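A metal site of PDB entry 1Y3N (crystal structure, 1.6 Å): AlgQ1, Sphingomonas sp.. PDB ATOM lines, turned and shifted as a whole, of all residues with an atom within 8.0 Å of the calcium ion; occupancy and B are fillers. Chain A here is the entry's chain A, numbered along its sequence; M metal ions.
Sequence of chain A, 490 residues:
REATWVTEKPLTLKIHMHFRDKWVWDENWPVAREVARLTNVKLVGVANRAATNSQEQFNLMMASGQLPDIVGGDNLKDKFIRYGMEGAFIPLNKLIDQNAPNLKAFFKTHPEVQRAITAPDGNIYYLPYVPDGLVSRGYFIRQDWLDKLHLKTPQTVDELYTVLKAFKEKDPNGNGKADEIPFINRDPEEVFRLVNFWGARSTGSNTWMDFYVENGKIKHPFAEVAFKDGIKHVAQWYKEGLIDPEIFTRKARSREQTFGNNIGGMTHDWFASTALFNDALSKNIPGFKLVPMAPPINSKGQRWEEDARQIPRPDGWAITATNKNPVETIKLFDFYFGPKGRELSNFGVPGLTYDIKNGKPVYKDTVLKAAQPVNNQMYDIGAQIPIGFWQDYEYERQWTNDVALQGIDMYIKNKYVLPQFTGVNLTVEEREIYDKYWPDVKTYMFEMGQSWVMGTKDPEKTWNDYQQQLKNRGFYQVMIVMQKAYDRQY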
ATOM      1  N   TRP A 145     -34.472   4.253 -23.879  1.00  0.00           N
ATOM      2  CA  TRP A 145     -33.556   4.992 -24.730  1.00  0.00           C
ATOM      3  C   TRP A 145     -34.366   5.910 -25.649  1.00  0.00           C
ATOM      4  O   TRP A 145     -33.951   7.033 -25.930  1.00  0.00           O
ATOM      5  CB  TRP A 145     -32.702   4.028 -25.550  1.00  0.00           C
ATOM      6  CG  TRP A 145     -31.531   3.468 -24.774  1.00  0.00           C
ATOM      7  CD1 TRP A 145     -31.297   3.583 -23.429  1.00  0.00           C
ATOM      8  CD2 TRP A 145     -30.440   2.715 -25.306  1.00  0.00           C
ATOM      9  NE1 TRP A 145     -30.126   2.948 -23.100  1.00  0.00           N
ATOM     10  CE2 TRP A 145     -29.579   2.402 -24.227  1.00  0.00           C
ATOM     11  CE3 TRP A 145     -30.109   2.271 -26.600  1.00  0.00           C
ATOM     12  CZ2 TRP A 145     -28.401   1.663 -24.402  1.00  0.00           C
ATOM     13  CZ3 TRP A 145     -28.938   1.534 -26.763  1.00  0.00           C
ATOM     14  CH2 TRP A 145     -28.100   1.238 -25.674  1.00  0.00           C
ATOM     15  N   PHE A 167     -29.250   5.968 -31.389  1.00  0.00           N
ATOM     16  CA  PHE A 167     -28.757   5.083 -30.335  1.00  0.00           C
ATOM     17  C   PHE A 167     -27.234   5.014 -30.430  1.00  0.00           C
ATOM     18  O   PHE A 167     -26.527   5.046 -29.422  1.00  0.00           O
ATOM     19  CB  PHE A 167     -29.310   3.668 -30.511  1.00  0.00           C
ATOM     20  CG  PHE A 167     -30.756   3.505 -30.120  1.00  0.00           C
ATOM     21  CD1 PHE A 167     -31.482   4.554 -29.574  1.00  0.00           C
ATOM     22  CD2 PHE A 167     -31.378   2.257 -30.275  1.00  0.00           C
ATOM     23  CE1 PHE A 167     -32.805   4.376 -29.188  1.00  0.00           C
ATOM     24  CE2 PHE A 167     -32.707   2.074 -29.884  1.00  0.00           C
ATOM     25  CZ  PHE A 167     -33.421   3.135 -29.349  1.00  0.00           C
ATOM     26  N   LYS A 168     -26.740   4.911 -31.653  1.00  0.00           N
ATOM     27  CA  LYS A 168     -25.301   4.813 -31.867  1.00  0.00           C
ATOM     28  C   LYS A 168     -24.518   6.095 -31.592  1.00  0.00           C
ATOM     29  O   LYS A 168     -23.443   6.043 -31.000  1.00  0.00           O
ATOM     30  CB  LYS A 168     -25.009   4.376 -33.303  1.00  0.00           C
ATOM     31  CG  LYS A 168     -23.520   4.288 -33.613  1.00  0.00           C
ATOM     32  CD  LYS A 168     -23.256   3.807 -35.017  1.00  0.00           C
ATOM     33  CE  LYS A 168     -21.771   3.565 -35.236  1.00  0.00           C
ATOM     34  NZ  LYS A 168     -20.980   4.804 -35.032  1.00  0.00           N
ATOM     35  N   GLU A 169     -25.062   7.236 -31.985  1.00  0.00           N
ATOM     36  CA  GLU A 169     -24.334   8.499 -31.825  1.00  0.00           C
ATOM     37  C   GLU A 169     -24.730   9.442 -30.689  1.00  0.00           C
ATOM     38  O   GLU A 169     -23.949  10.324 -30.337  1.00  0.00           O
ATOM     39  CB  GLU A 169     -24.421   9.306 -33.121  1.00  0.00           C
ATOM     40  CG  GLU A 169     -24.200   8.498 -34.383  1.00  0.00           C
ATOM     41  CD  GLU A 169     -24.402   9.335 -35.631  1.00  0.00           C
ATOM     42  OE1 GLU A 169     -25.377  10.120 -35.653  1.00  0.00           O
ATOM     43  OE2 GLU A 169     -23.615   9.203 -36.584  1.00  0.00           O
ATOM     44  N   LYS A 170     -25.909   9.246 -30.114  1.00  0.00           N
ATOM     45  CA  LYS A 170     -26.362  10.153 -29.060  1.00  0.00           C
ATOM     46  C   LYS A 170     -26.185   9.733 -27.616  1.00  0.00           C
ATOM     47  O   LYS A 170     -26.820  10.285 -26.721  1.00  0.00           O
ATOM     48  CB  LYS A 170     -27.819  10.528 -29.334  1.00  0.00           C
ATOM     49  CG  LYS A 170     -28.047  11.015 -30.765  1.00  0.00           C
ATOM     50  CD  LYS A 170     -27.173  12.213 -31.099  1.00  0.00           C
ATOM     51  CE  LYS A 170     -27.698  13.481 -30.437  1.00  0.00           C
ATOM     52  NZ  LYS A 170     -29.062  13.798 -30.936  1.00  0.00           N
ATOM     53  N   ASP A 171     -25.320   8.746 -27.383  1.00  0.00           N
ATOM     54  CA  ASP A 171     -25.011   8.315 -26.021  1.00  0.00           C
ATOM     55  C   ASP A 171     -26.228   8.150 -25.100  1.00  0.00           C
ATOM     56  O   ASP A 171     -26.314   8.796 -24.052  1.00  0.00           O
ATOM     57  CB  ASP A 171     -24.040   9.345 -25.421  1.00  0.00           C
ATOM     58  CG  ASP A 171     -23.490   8.920 -24.079  1.00  0.00           C
ATOM     59  OD1 ASP A 171     -23.189   9.829 -23.274  1.00  0.00           O
ATOM     60  OD2 ASP A 171     -23.339   7.708 -23.826  1.00  0.00           O
ATOM     61  N   PRO A 172     -27.183   7.286 -25.481  1.00  0.00           N
ATOM     62  CA  PRO A 172     -28.354   7.115 -24.623  1.00  0.00           C
ATOM     63  C   PRO A 172     -28.064   6.579 -23.209  1.00  0.00           C
ATOM     64  O   PRO A 172     -28.811   6.897 -22.276  1.00  0.00           O
ATOM     65  CB  PRO A 172     -29.254   6.197 -25.443  1.00  0.00           C
ATOM     66  CG  PRO A 172     -28.290   5.401 -26.244  1.00  0.00           C
ATOM     67  CD  PRO A 172     -27.285   6.450 -26.690  1.00  0.00           C
ATOM     68  N   ASN A 173     -27.012   5.778 -23.032  1.00  0.00           N
ATOM     69  CA  ASN A 173     -26.725   5.296 -21.675  1.00  0.00           C
ATOM     70  C   ASN A 173     -25.981   6.367 -20.869  1.00  0.00           C
ATOM     71  O   ASN A 173     -25.599   6.157 -19.725  1.00  0.00           O
ATOM     72  CB  ASN A 173     -25.955   3.960 -21.677  1.00  0.00           C
ATOM     73  CG  ASN A 173     -24.564   4.050 -22.272  1.00  0.00           C
ATOM     74  OD1 ASN A 173     -23.928   5.103 -22.260  1.00  0.00           O
ATOM     75  ND2 ASN A 173     -24.068   2.919 -22.774  1.00  0.00           N
ATOM     76  N   GLY A 174     -25.794   7.529 -21.501  1.00  0.00           N
ATOM     77  CA  GLY A 174     -25.163   8.674 -20.869  1.00  0.00           C
ATOM     78  C   GLY A 174     -23.795   8.597 -20.216  1.00  0.00           C
ATOM     79  O   GLY A 174     -23.509   9.381 -19.322  1.00  0.00           O
ATOM     80  N   ASN A 175     -22.942   7.676 -20.657  1.00  0.00           N
ATOM     81  CA  ASN A 175     -21.618   7.569 -20.063  1.00  0.00           C
ATOM     82  C   ASN A 175     -20.543   8.333 -20.843  1.00  0.00           C
ATOM     83  O   ASN A 175     -19.349   8.175 -20.583  1.00  0.00           O
ATOM     84  CB  ASN A 175     -21.218   6.087 -19.901  1.00  0.00           C
ATOM     85  CG  ASN A 175     -21.097   5.351 -21.232  1.00  0.00           C
ATOM     86  OD1 ASN A 175     -20.906   4.131 -21.247  1.00  0.00           O
ATOM     87  ND2 ASN A 175     -21.189   6.073 -22.335  1.00  0.00           N
ATOM     88  N   GLY A 176     -20.972   9.164 -21.775  1.00  0.00           N
ATOM     89  CA  GLY A 176     -20.045   9.963 -22.573  1.00  0.00           C
ATOM     90  C   GLY A 176     -19.212   9.189 -23.583  1.00  0.00           C
ATOM     91  O   GLY A 176     -18.310   9.758 -24.210  1.00  0.00           O
ATOM     92  N   LYS A 177     -19.511   7.910 -23.758  1.00  0.00           N
ATOM     93  CA  LYS A 177     -18.781   7.082 -24.702  1.00  0.00           C
ATOM     94  C   LYS A 177     -19.688   6.492 -25.771  1.00  0.00           C
ATOM     95  O   LYS A 177     -20.868   6.234 -25.524  1.00  0.00           O
ATOM     96  CB  LYS A 177     -18.056   5.940 -23.974  1.00  0.00           C
ATOM     97  CG  LYS A 177     -17.096   6.396 -22.892  1.00  0.00           C
ATOM     98  CD  LYS A 177     -16.283   5.240 -22.349  1.00  0.00           C
ATOM     99  CE  LYS A 177     -17.166   4.166 -21.724  1.00  0.00           C
ATOM    100  NZ  LYS A 177     -16.363   2.991 -21.264  1.00  0.00           N
ATOM    101  N   ALA A 178     -19.137   6.291 -26.958  1.00  0.00           N
ATOM    102  CA  ALA A 178     -19.878   5.719 -28.079  1.00  0.00           C
ATOM    103  C   ALA A 178     -19.710   4.206 -28.002  1.00  0.00           C
ATOM    104  O   ALA A 178     -19.006   3.602 -28.821  1.00  0.00           O
ATOM    105  CB  ALA A 178     -19.349   6.260 -29.403  1.00  0.00           C
ATOM    106  N   ASP A 179     -20.340   3.607 -27.004  1.00  0.00           N
ATOM    107  CA  ASP A 179     -20.270   2.163 -26.786  1.00  0.00           C
ATOM    108  C   ASP A 179     -21.564   1.439 -27.163  1.00  0.00           C
ATOM    109  O   ASP A 179     -21.594   0.208 -27.196  1.00  0.00           O
ATOM    110  CB  ASP A 179     -19.912   1.856 -25.319  1.00  0.00           C
ATOM    111  CG  ASP A 179     -20.885   2.484 -24.322  1.00  0.00           C
ATOM    112  OD1 ASP A 179     -20.848   2.080 -23.139  1.00  0.00           O
ATOM    113  OD2 ASP A 179     -21.664   3.386 -24.708  1.00  0.00           O
ATOM    114  N   GLU A 180     -22.605   2.199 -27.457  1.00  0.00           N
ATOM    115  CA  GLU A 180     -23.895   1.627 -27.820  1.00  0.00           C
ATOM    116  C   GLU A 180     -23.879   0.827 -29.133  1.00  0.00           C
ATOM    117  O   GLU A 180     -23.236   1.224 -30.105  1.00  0.00           O
ATOM    118  CB  GLU A 180     -24.963   2.722 -27.917  1.00  0.00           C
ATOM    119  CG  GLU A 180     -25.372   3.352 -26.593  1.00  0.00           C
ATOM    120  CD  GLU A 180     -24.438   4.456 -26.103  1.00  0.00           C
ATOM    121  OE1 GLU A 180     -24.751   5.037 -25.044  1.00  0.00           O
ATOM    122  OE2 GLU A 180     -23.418   4.737 -26.765  1.00  0.00           O
ATOM    123  N   ILE A 181     -24.584  -0.298 -29.131  1.00  0.00           N
ATOM    124  CA  ILE A 181     -24.708  -1.158 -30.300  1.00  0.00           C
ATOM    125  C   ILE A 181     -26.215  -1.222 -30.533  1.00  0.00           C
ATOM    126  O   ILE A 181     -26.930  -1.934 -29.829  1.00  0.00           O
ATOM    127  CB  ILE A 181     -24.167  -2.567 -30.018  1.00  0.00           C
ATOM    128  CG1 ILE A 181     -22.717  -2.470 -29.531  1.00  0.00           C
ATOM    129  CG2 ILE A 181     -24.262  -3.417 -31.270  1.00  0.00           C
ATOM    130  CD1 ILE A 181     -22.102  -3.823 -29.201  1.00  0.00           C
ATOM    131  N   ASN A 262     -25.715  -2.540 -20.681  1.00  0.00           N
ATOM    132  CA  ASN A 262     -26.468  -1.371 -21.145  1.00  0.00           C
ATOM    133  C   ASN A 262     -25.933  -0.741 -22.446  1.00  0.00           C
ATOM    134  O   ASN A 262     -25.781   0.479 -22.542  1.00  0.00           O
ATOM    135  CB  ASN A 262     -26.520  -0.320 -20.030  1.00  0.00           C
ATOM    136  CG  ASN A 262     -27.617   0.713 -20.238  1.00  0.00           C
ATOM    137  OD1 ASN A 262     -28.507   0.528 -21.064  1.00  0.00           O
ATOM    138  ND2 ASN A 262     -27.571   1.807 -19.471  1.00  0.00           N
ATOM    139  N   ILE A 263     -25.648  -1.580 -23.437  1.00  0.00           N
ATOM    140  CA  ILE A 263     -25.180  -1.101 -24.728  1.00  0.00           C
ATOM    141  C   ILE A 263     -26.011  -1.613 -25.904  1.00  0.00           C
ATOM    142  O   ILE A 263     -25.805  -1.179 -27.046  1.00  0.00           O
ATOM    143  CB  ILE A 263     -23.684  -1.459 -24.998  1.00  0.00           C
ATOM    144  CG1 ILE A 263     -23.444  -2.953 -24.790  1.00  0.00           C
ATOM    145  CG2 ILE A 263     -22.792  -0.605 -24.110  1.00  0.00           C
ATOM    146  CD1 ILE A 263     -22.005  -3.364 -25.050  1.00  0.00           C
HETATM  147 CA    CA M   1     -22.610   5.601 -24.251  1.00  0.00          CA
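Of the 18 residues printed, 6 come within 4 Å of the calcium ion.
OD2 of Asp 171 lies close to N of Gly 174, 3.4 Å away.
OD1 of Asp 171 is in hydrogen-bond range of N of Gly 176 (2.8 Å).
ND2 of Asn 173 sits at hydrogen-bond distance from O of Asn 262 (3.0 Å).
O of Lys 177 is bound to the calcium ion (2.2 Å).
The calcium ion is bound by OD2 of Asp 171 (2.3 Å).
The calcium ion is bound by OE1 of Glu 180, at 2.4 Å.
The side-chain amide nitrogen (ND2) of Asn 175 binds the calcium ion (2.4 Å).
The calcium ion is bound by OD1 of Asn 173 (2.4 Å).
OD2 of Asp 179 is bound to the calcium ion (2.5 Å).
The side-chain carboxylate (OE2) of Glu 180 is bound to the calcium ion, at 2.8 Å.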
